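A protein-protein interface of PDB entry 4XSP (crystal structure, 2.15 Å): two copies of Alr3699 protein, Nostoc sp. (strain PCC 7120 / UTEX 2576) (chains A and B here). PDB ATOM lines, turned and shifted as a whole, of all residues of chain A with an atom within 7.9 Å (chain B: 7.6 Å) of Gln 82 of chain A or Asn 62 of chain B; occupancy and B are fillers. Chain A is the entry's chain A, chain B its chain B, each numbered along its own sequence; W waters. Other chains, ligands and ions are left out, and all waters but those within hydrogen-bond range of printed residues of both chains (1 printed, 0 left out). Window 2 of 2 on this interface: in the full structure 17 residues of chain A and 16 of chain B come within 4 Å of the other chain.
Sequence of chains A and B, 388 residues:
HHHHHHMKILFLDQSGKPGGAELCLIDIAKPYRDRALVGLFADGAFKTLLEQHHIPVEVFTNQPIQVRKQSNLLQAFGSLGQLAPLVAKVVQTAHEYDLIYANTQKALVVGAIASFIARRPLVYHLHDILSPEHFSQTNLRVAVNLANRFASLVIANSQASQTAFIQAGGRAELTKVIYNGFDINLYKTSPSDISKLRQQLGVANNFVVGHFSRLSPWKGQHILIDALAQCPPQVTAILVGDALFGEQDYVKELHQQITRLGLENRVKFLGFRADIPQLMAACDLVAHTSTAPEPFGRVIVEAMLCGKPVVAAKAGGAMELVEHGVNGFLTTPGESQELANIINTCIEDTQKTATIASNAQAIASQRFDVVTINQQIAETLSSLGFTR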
ATOM      1  N   ASN A  62     -32.365  22.014 -20.417  1.00  0.00           N
ATOM      2  CA  ASN A  62     -31.070  22.571 -20.023  1.00  0.00           C
ATOM      3  C   ASN A  62     -30.931  24.085 -20.276  1.00  0.00           C
ATOM      4  O   ASN A  62     -29.821  24.604 -20.282  1.00  0.00           O
ATOM      5  CB  ASN A  62     -29.938  21.822 -20.757  1.00  0.00           C
ATOM      6  CG  ASN A  62     -29.270  20.778 -19.895  1.00  0.00           C
ATOM      7  OD1 ASN A  62     -29.314  20.844 -18.669  1.00  0.00           O
ATOM      8  ND2 ASN A  62     -28.603  19.821 -20.539  1.00  0.00           N
ATOM      9  N   PRO A  64     -30.714  27.989 -19.536  1.00  0.00           N
ATOM     10  CA  PRO A  64     -30.366  28.865 -18.394  1.00  0.00           C
ATOM     11  C   PRO A  64     -31.527  29.686 -17.816  1.00  0.00           C
ATOM     12  O   PRO A  64     -31.537  29.952 -16.612  1.00  0.00           O
ATOM     13  CB  PRO A  64     -29.298  29.800 -18.982  1.00  0.00           C
ATOM     14  CG  PRO A  64     -28.676  29.028 -20.096  1.00  0.00           C
ATOM     15  CD  PRO A  64     -29.711  28.072 -20.621  1.00  0.00           C
ATOM     16  N   SER A  79     -26.781  29.035  -7.575  1.00  0.00           N
ATOM     17  CA  SER A  79     -25.459  28.613  -8.014  1.00  0.00           C
ATOM     18  C   SER A  79     -25.595  27.434  -8.961  1.00  0.00           C
ATOM     19  O   SER A  79     -25.090  27.462 -10.082  1.00  0.00           O
ATOM     20  CB  SER A  79     -24.605  28.218  -6.810  1.00  0.00           C
ATOM     21  OG  SER A  79     -25.246  27.213  -6.043  1.00  0.00           O
ATOM     22  N   LEU A  80     -26.297  26.406  -8.499  1.00  0.00           N
ATOM     23  CA  LEU A  80     -26.630  25.246  -9.328  1.00  0.00           C
ATOM     24  C   LEU A  80     -27.391  25.658 -10.606  1.00  0.00           C
ATOM     25  O   LEU A  80     -27.248  25.021 -11.668  1.00  0.00           O
ATOM     26  CB  LEU A  80     -27.460  24.254  -8.492  1.00  0.00           C
ATOM     27  CG  LEU A  80     -27.834  22.871  -9.037  1.00  0.00           C
ATOM     28  CD1 LEU A  80     -26.614  21.981  -9.321  1.00  0.00           C
ATOM     29  CD2 LEU A  80     -28.787  22.235  -8.031  1.00  0.00           C
ATOM     30  N   GLY A  81     -28.186  26.729 -10.499  1.00  0.00           N
ATOM     31  CA  GLY A  81     -28.914  27.283 -11.642  1.00  0.00           C
ATOM     32  C   GLY A  81     -28.071  27.321 -12.900  1.00  0.00           C
ATOM     33  O   GLY A  81     -28.492  26.881 -13.959  1.00  0.00           O
ATOM     34  N   GLN A  82     -26.853  27.824 -12.783  1.00  0.00           N
ATOM     35  CA  GLN A  82     -25.992  27.948 -13.952  1.00  0.00           C
ATOM     36  C   GLN A  82     -25.118  26.715 -14.184  1.00  0.00           C
ATOM     37  O   GLN A  82     -24.888  26.336 -15.327  1.00  0.00           O
ATOM     38  CB  GLN A  82     -25.179  29.236 -13.853  1.00  0.00           C
ATOM     39  CG  GLN A  82     -26.024  30.458 -14.203  1.00  0.00           C
ATOM     40  CD  GLN A  82     -25.557  31.733 -13.530  1.00  0.00           C
ATOM     41  OE1 GLN A  82     -24.528  31.759 -12.854  1.00  0.00           O
ATOM     42  NE2 GLN A  82     -26.322  32.805 -13.708  1.00  0.00           N
ATOM     43  N   LEU A  83     -24.657  26.081 -13.107  1.00  0.00           N
ATOM     44  CA  LEU A  83     -23.814  24.872 -13.218  1.00  0.00           C
ATOM     45  C   LEU A  83     -24.505  23.714 -13.962  1.00  0.00           C
ATOM     46  O   LEU A  83     -23.885  23.011 -14.764  1.00  0.00           O
ATOM     47  CB  LEU A  83     -23.393  24.392 -11.829  1.00  0.00           C
ATOM     48  CG  LEU A  83     -22.544  25.347 -10.980  1.00  0.00           C
ATOM     49  CD1 LEU A  83     -22.421  24.862  -9.540  1.00  0.00           C
ATOM     50  CD2 LEU A  83     -21.172  25.540 -11.603  1.00  0.00           C
ATOM     51  N   ALA A  84     -25.792  23.523 -13.683  1.00  0.00           N
ATOM     52  CA  ALA A  84     -26.570  22.421 -14.260  1.00  0.00           C
ATOM     53  C   ALA A  84     -28.061  22.798 -14.234  1.00  0.00           C
ATOM     54  O   ALA A  84     -28.758  22.466 -13.265  1.00  0.00           O
ATOM     55  CB  ALA A  84     -26.326  21.144 -13.463  1.00  0.00           C
ATOM     56  N   PRO A  85     -28.541  23.503 -15.287  1.00  0.00           N
ATOM     57  CA  PRO A  85     -29.897  24.088 -15.335  1.00  0.00           C
ATOM     58  C   PRO A  85     -31.014  23.064 -15.095  1.00  0.00           C
ATOM     59  O   PRO A  85     -31.830  23.270 -14.205  1.00  0.00           O
ATOM     60  CB  PRO A  85     -29.998  24.669 -16.765  1.00  0.00           C
ATOM     61  CG  PRO A  85     -28.594  24.716 -17.276  1.00  0.00           C
ATOM     62  CD  PRO A  85     -27.856  23.613 -16.590  1.00  0.00           C
ATOM     63  N   LEU A  86     -31.015  21.988 -15.888  1.00  0.00           N
ATOM     64  CA  LEU A  86     -31.986  20.893 -15.776  1.00  0.00           C
ATOM     65  C   LEU A  86     -32.105  20.392 -14.334  1.00  0.00           C
ATOM     66  O   LEU A  86     -33.162  20.483 -13.705  1.00  0.00           O
ATOM     67  CB  LEU A  86     -31.578  19.741 -16.690  1.00  0.00           C
ATOM     68  CG  LEU A  86     -32.465  18.494 -16.669  1.00  0.00           C
ATOM     69  CD1 LEU A  86     -33.890  18.861 -17.026  1.00  0.00           C
ATOM     70  CD2 LEU A  86     -31.912  17.440 -17.622  1.00  0.00           C
ATOM     71  N   ALA A  88     -31.010  21.699 -11.665  1.00  0.00           N
ATOM     72  CA  ALA A  88     -31.393  22.766 -10.744  1.00  0.00           C
ATOM     73  C   ALA A  88     -32.905  22.981 -10.734  1.00  0.00           C
ATOM     74  O   ALA A  88     -33.511  23.229  -9.686  1.00  0.00           O
ATOM     75  CB  ALA A  88     -30.691  24.060 -11.125  1.00  0.00           C
ATOM     76  N   PHE B  41     -14.019  26.343 -13.385  1.00  0.00           N
ATOM     77  CA  PHE B  41     -15.346  26.504 -13.974  1.00  0.00           C
ATOM     78  C   PHE B  41     -15.496  27.838 -14.738  1.00  0.00           C
ATOM     79  O   PHE B  41     -16.597  28.231 -15.121  1.00  0.00           O
ATOM     80  CB  PHE B  41     -16.417  26.411 -12.867  1.00  0.00           C
ATOM     81  CG  PHE B  41     -16.463  25.072 -12.144  1.00  0.00           C
ATOM     82  CD1 PHE B  41     -15.772  23.968 -12.604  1.00  0.00           C
ATOM     83  CD2 PHE B  41     -17.265  24.916 -11.018  1.00  0.00           C
ATOM     84  CE1 PHE B  41     -15.844  22.762 -11.946  1.00  0.00           C
ATOM     85  CE2 PHE B  41     -17.336  23.705 -10.356  1.00  0.00           C
ATOM     86  CZ  PHE B  41     -16.631  22.631 -10.828  1.00  0.00           C
ATOM     87  N   VAL B  59     -10.279  24.172 -18.192  1.00  0.00           N
ATOM     88  CA  VAL B  59     -11.555  24.864 -17.925  1.00  0.00           C
ATOM     89  C   VAL B  59     -12.727  23.988 -18.361  1.00  0.00           C
ATOM     90  O   VAL B  59     -12.771  23.528 -19.478  1.00  0.00           O
ATOM     91  CB  VAL B  59     -11.651  26.230 -18.631  1.00  0.00           C
ATOM     92  CG1 VAL B  59     -12.999  26.883 -18.350  1.00  0.00           C
ATOM     93  CG2 VAL B  59     -10.535  27.140 -18.178  1.00  0.00           C
ATOM     94  N   PHE B  60     -13.645  23.727 -17.439  1.00  0.00           N
ATOM     95  CA  PHE B  60     -14.804  22.899 -17.711  1.00  0.00           C
ATOM     96  C   PHE B  60     -16.019  23.813 -17.894  1.00  0.00           C
ATOM     97  O   PHE B  60     -16.273  24.708 -17.081  1.00  0.00           O
ATOM     98  CB  PHE B  60     -15.023  21.917 -16.570  1.00  0.00           C
ATOM     99  CG  PHE B  60     -13.967  20.855 -16.476  1.00  0.00           C
ATOM    100  CD1 PHE B  60     -12.820  21.052 -15.715  1.00  0.00           C
ATOM    101  CD2 PHE B  60     -14.110  19.659 -17.161  1.00  0.00           C
ATOM    102  CE1 PHE B  60     -11.839  20.080 -15.651  1.00  0.00           C
ATOM    103  CE2 PHE B  60     -13.148  18.667 -17.077  1.00  0.00           C
ATOM    104  CZ  PHE B  60     -12.008  18.882 -16.321  1.00  0.00           C
ATOM    105  N   THR B  61     -16.741  23.611 -18.987  1.00  0.00           N
ATOM    106  CA  THR B  61     -17.924  24.430 -19.294  1.00  0.00           C
ATOM    107  C   THR B  61     -19.155  23.551 -19.504  1.00  0.00           C
ATOM    108  O   THR B  61     -19.062  22.319 -19.470  1.00  0.00           O
ATOM    109  CB  THR B  61     -17.696  25.270 -20.567  1.00  0.00           C
ATOM    110  OG1 THR B  61     -17.518  24.389 -21.687  1.00  0.00           O
ATOM    111  CG2 THR B  61     -16.469  26.151 -20.402  1.00  0.00           C
ATOM    112  N   ASN B  62     -20.295  24.201 -19.739  1.00  0.00           N
ATOM    113  CA  ASN B  62     -21.544  23.507 -20.047  1.00  0.00           C
ATOM    114  C   ASN B  62     -21.878  23.337 -21.535  1.00  0.00           C
ATOM    115  O   ASN B  62     -22.916  22.766 -21.868  1.00  0.00           O
ATOM    116  CB  ASN B  62     -22.711  24.176 -19.314  1.00  0.00           C
ATOM    117  CG  ASN B  62     -23.032  23.488 -17.999  1.00  0.00           C
ATOM    118  OD1 ASN B  62     -23.312  22.280 -17.957  1.00  0.00           O
ATOM    119  ND2 ASN B  62     -22.992  24.248 -16.917  1.00  0.00           N
ATOM    120  N   GLN B  63     -21.010  23.788 -22.436  1.00  0.00           N
ATOM    121  CA  GLN B  63     -21.206  23.452 -23.847  1.00  0.00           C
ATOM    122  C   GLN B  63     -21.107  21.920 -23.990  1.00  0.00           C
ATOM    123  O   GLN B  63     -20.583  21.258 -23.093  1.00  0.00           O
ATOM    124  CB  GLN B  63     -20.186  24.171 -24.731  1.00  0.00           C
ATOM    125  CG  GLN B  63     -18.777  23.615 -24.640  1.00  0.00           C
ATOM    126  CD  GLN B  63     -17.845  24.227 -25.668  1.00  0.00           C
ATOM    127  OE1 GLN B  63     -17.902  25.434 -25.936  1.00  0.00           O
ATOM    128  NE2 GLN B  63     -16.974  23.400 -26.246  1.00  0.00           N
ATOM    129  N   PRO B  64     -21.613  21.348 -25.098  1.00  0.00           N
ATOM    130  CA  PRO B  64     -21.670  19.888 -25.161  1.00  0.00           C
ATOM    131  C   PRO B  64     -20.624  19.246 -26.065  1.00  0.00           C
ATOM    132  O   PRO B  64     -20.416  18.032 -25.976  1.00  0.00           O
ATOM    133  CB  PRO B  64     -23.083  19.629 -25.703  1.00  0.00           C
ATOM    134  CG  PRO B  64     -23.616  20.972 -26.156  1.00  0.00           C
ATOM    135  CD  PRO B  64     -22.474  21.940 -26.128  1.00  0.00           C
ATOM    136  N   LEU B  80     -25.413  11.495 -18.912  1.00  0.00           N
ATOM    137  CA  LEU B  80     -25.202  12.748 -18.165  1.00  0.00           C
ATOM    138  C   LEU B  80     -24.468  13.830 -19.008  1.00  0.00           C
ATOM    139  O   LEU B  80     -24.598  15.040 -18.764  1.00  0.00           O
ATOM    140  CB  LEU B  80     -24.437  12.429 -16.867  1.00  0.00           C
ATOM    141  CG  LEU B  80     -24.290  13.487 -15.768  1.00  0.00           C
ATOM    142  CD1 LEU B  80     -25.629  13.995 -15.242  1.00  0.00           C
ATOM    143  CD2 LEU B  80     -23.437  12.893 -14.654  1.00  0.00           C
ATOM    144  N   GLY B  81     -23.717  13.393 -20.014  1.00  0.00           N
ATOM    145  CA  GLY B  81     -23.106  14.315 -20.982  1.00  0.00           C
ATOM    146  C   GLY B  81     -24.109  15.293 -21.565  1.00  0.00           C
ATOM    147  O   GLY B  81     -23.808  16.469 -21.752  1.00  0.00           O
ATOM    148  N   GLN B  82     -25.319  14.811 -21.814  1.00  0.00           N
ATOM    149  CA  GLN B  82     -26.377  15.648 -22.359  1.00  0.00           C
ATOM    150  C   GLN B  82     -27.162  16.328 -21.236  1.00  0.00           C
ATOM    151  O   GLN B  82     -27.591  17.465 -21.370  1.00  0.00           O
ATOM    152  CB  GLN B  82     -27.311  14.789 -23.210  1.00  0.00           C
ATOM    153  CG  GLN B  82     -26.575  13.899 -24.193  1.00  0.00           C
ATOM    154  CD  GLN B  82     -27.493  12.900 -24.862  1.00  0.00           C
ATOM    155  OE1 GLN B  82     -27.533  11.721 -24.483  1.00  0.00           O
ATOM    156  NE2 GLN B  82     -28.254  13.366 -25.858  1.00  0.00           N
ATOM    157  N   LEU B  83     -27.334  15.628 -20.116  1.00  0.00           N
ATOM    158  CA  LEU B  83     -28.211  16.111 -19.054  1.00  0.00           C
ATOM    159  C   LEU B  83     -27.563  17.229 -18.279  1.00  0.00           C
ATOM    160  O   LEU B  83     -28.257  18.160 -17.865  1.00  0.00           O
ATOM    161  CB  LEU B  83     -28.586  14.975 -18.108  1.00  0.00           C
ATOM    162  CG  LEU B  83     -29.204  13.732 -18.778  1.00  0.00           C
ATOM    163  CD1 LEU B  83     -29.460  12.630 -17.757  1.00  0.00           C
ATOM    164  CD2 LEU B  83     -30.483  14.080 -19.541  1.00  0.00           C
ATOM    165  N   ALA B  84     -26.239  17.134 -18.080  1.00  0.00           N
ATOM    166  CA  ALA B  84     -25.469  18.139 -17.317  1.00  0.00           C
ATOM    167  C   ALA B  84     -23.995  18.103 -17.746  1.00  0.00           C
ATOM    168  O   ALA B  84     -23.172  17.443 -17.101  1.00  0.00           O
ATOM    169  CB  ALA B  84     -25.605  17.888 -15.819  1.00  0.00           C
ATOM    170  N   PRO B  85     -23.663  18.790 -18.859  1.00  0.00           N
ATOM    171  CA  PRO B  85     -22.352  18.605 -19.522  1.00  0.00           C
ATOM    172  C   PRO B  85     -21.143  18.894 -18.629  1.00  0.00           C
ATOM    173  O   PRO B  85     -20.190  18.113 -18.581  1.00  0.00           O
ATOM    174  CB  PRO B  85     -22.406  19.594 -20.709  1.00  0.00           C
ATOM    175  CG  PRO B  85     -23.871  19.847 -20.948  1.00  0.00           C
ATOM    176  CD  PRO B  85     -24.561  19.684 -19.623  1.00  0.00           C
ATOM    177  N   LEU B  86     -21.190  20.033 -17.951  1.00  0.00           N
ATOM    178  CA  LEU B  86     -20.162  20.397 -17.001  1.00  0.00           C
ATOM    179  C   LEU B  86     -19.906  19.228 -16.022  1.00  0.00           C
ATOM    180  O   LEU B  86     -18.798  18.672 -16.012  1.00  0.00           O
ATOM    181  CB  LEU B  86     -20.553  21.706 -16.299  1.00  0.00           C
ATOM    182  CG  LEU B  86     -19.860  22.097 -14.988  1.00  0.00           C
ATOM    183  CD1 LEU B  86     -18.343  22.147 -15.119  1.00  0.00           C
ATOM    184  CD2 LEU B  86     -20.408  23.434 -14.503  1.00  0.00           C
ATOM    185  N   VAL B  87     -20.936  18.816 -15.265  1.00  0.00           N
ATOM    186  CA  VAL B  87     -20.813  17.690 -14.309  1.00  0.00           C
ATOM    187  C   VAL B  87     -20.244  16.464 -14.990  1.00  0.00           C
ATOM    188  O   VAL B  87     -19.366  15.788 -14.446  1.00  0.00           O
ATOM    189  CB  VAL B  87     -22.175  17.318 -13.667  1.00  0.00           C
ATOM    190  CG1 VAL B  87     -22.141  15.945 -12.997  1.00  0.00           C
ATOM    191  CG2 VAL B  87     -22.593  18.373 -12.667  1.00  0.00           C
ATOM    192  N   ALA B  88     -20.747  16.179 -16.188  1.00  0.00           N
ATOM    193  CA  ALA B  88     -20.326  14.994 -16.926  1.00  0.00           C
ATOM    194  C   ALA B  88     -18.836  14.999 -17.275  1.00  0.00           C
ATOM    195  O   ALA B  88     -18.169  13.971 -17.181  1.00  0.00           O
ATOM    196  CB  ALA B  88     -21.149  14.848 -18.187  1.00  0.00           C
ATOM    197  N   LYS B  89     -18.332  16.142 -17.724  1.00  0.00           N
ATOM    198  CA  LYS B  89     -16.898  16.268 -18.004  1.00  0.00           C
ATOM    199  C   LYS B  89     -16.046  16.084 -16.710  1.00  0.00           C
ATOM    200  O   LYS B  89     -15.023  15.428 -16.729  1.00  0.00           O
ATOM    201  CB  LYS B  89     -16.608  17.624 -18.641  1.00  0.00           C
ATOM    202  CG  LYS B  89     -17.154  17.809 -20.054  1.00  0.00           C
ATOM    203  CD  LYS B  89     -17.310  19.297 -20.363  1.00  0.00           C
ATOM    204  CE  LYS B  89     -18.079  19.581 -21.646  1.00  0.00           C
ATOM    205  NZ  LYS B  89     -18.213  21.040 -21.835  1.00  0.00           N
ATOM    206  N   LYS B 106     -18.992  26.205  -5.238  1.00  0.00           N
ATOM    207  CA  LYS B 106     -19.475  25.556  -6.447  1.00  0.00           C
ATOM    208  C   LYS B 106     -18.690  24.292  -6.779  1.00  0.00           C
ATOM    209  O   LYS B 106     -19.254  23.324  -7.321  1.00  0.00           O
ATOM    210  CB  LYS B 106     -19.455  26.527  -7.627  1.00  0.00           C
ATOM    211  CG  LYS B 106     -20.514  27.607  -7.484  1.00  0.00           C
ATOM    212  CD  LYS B 106     -20.566  28.580  -8.645  1.00  0.00           C
ATOM    213  CE  LYS B 106     -21.410  29.793  -8.271  1.00  0.00           C
ATOM    214  NZ  LYS B 106     -21.133  30.961  -9.153  1.00  0.00           N
HETATM  215  O   HOH W   1     -28.155  20.265 -16.409  1.00  0.00           O
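O of Gln 82 of chain A lies within hydrogen-bond range of ND2 of Asn 62 of chain B. O of Leu 83 of chain A is in hydrogen-bond range of ND2 of Asn 62 of chain B (2.6 Å). The backbone carbonyl oxygen of Gln 82 of chain B lies within hydrogen-bond range of the side-chain amide nitrogen of Asn 62 of chain A (2.7 Å). O of Leu 83 of chain B sits close to OD1 of Asn 62 of chain A (3.0 Å).
O of Thr 61 of chain B lies close to N of Leu 86 of chain B, at 3.5 Å. N of Leu 86 of chain B lies within hydrogen-bond range of OD1 of Asn 62 of chain B. N of Leu 86 of chain A sits close to OD1 of Asn 62 of chain A.
Among the printed residues, merely in contact across the chains: Ser 79 of chain A with Lys 106 of chain B (3.9 Å), Leu 83 of chain A with Phe 41 of chain B (3.9995 Å), Leu 83 of chain A with Leu 86 of chain B (3.5 Å), Leu 83 of chain A with Lys 106 of chain B (3.9 Å) and Leu 86 of chain A with Leu 83 of chain B (3.7 Å).
Of the printed residues of chain B, Ser 79 of chain A touches Lys 106 (3.9 Å). Gln 82 of chain A touches one residue of chain B. Of the printed residues of chain B, Leu 83 of chain A touches Phe 41, Asn 62, Leu 86 and Lys 106. Of the printed residues of chain A, Gln 82 of chain B touches Asn 62 (2.7 Å). Of the printed residues of chain A, Leu 83 of chain B touches Asn 62 and Leu 86. The nearest residue of chain B that does not touch Gln 82 of chain A is Lys 106 of chain B (5.1 Å). The nearest printed residue of chain B that does not touch Ser 79 of chain A is Leu 86 of chain B (7.6 Å).
Of the 18 printed residues of chain B, 6 touch a printed residue of chain A. Of the 11 printed residues of chain A, 5 touch a printed residue of chain B. Hydrophobic or aromatic side chains of chain A that line the printed part of chain B: Leu 83 and Leu 86. Along chain A the printed residues that touch a printed residue of chain B span positions 62 to 86. Among the printed residues, 9 pairs touch across the chains.
Asn 62 of chain A touches Gln 82 of chain B, and with the chains exchanged Gln 82 of chain A touches Asn 62 of chain B. Asn 62 of chain A touches Leu 83 of chain B, and with the chains exchanged Leu 83 of chain A touches Asn 62 of chain B. Leu 83 of chain A touches Leu 86 of chain B, and with the chains exchanged Leu 86 of chain A touches Leu 83 of chain B. 10 positions are printed for both chains.
Water W1 lies within hydrogen-bond range of the backbone carbonyl oxygen of Leu 83 of chain B, the side-chain amide oxygen of Asn 62 of chain A and the backbone NH of Leu 86 of chain A.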
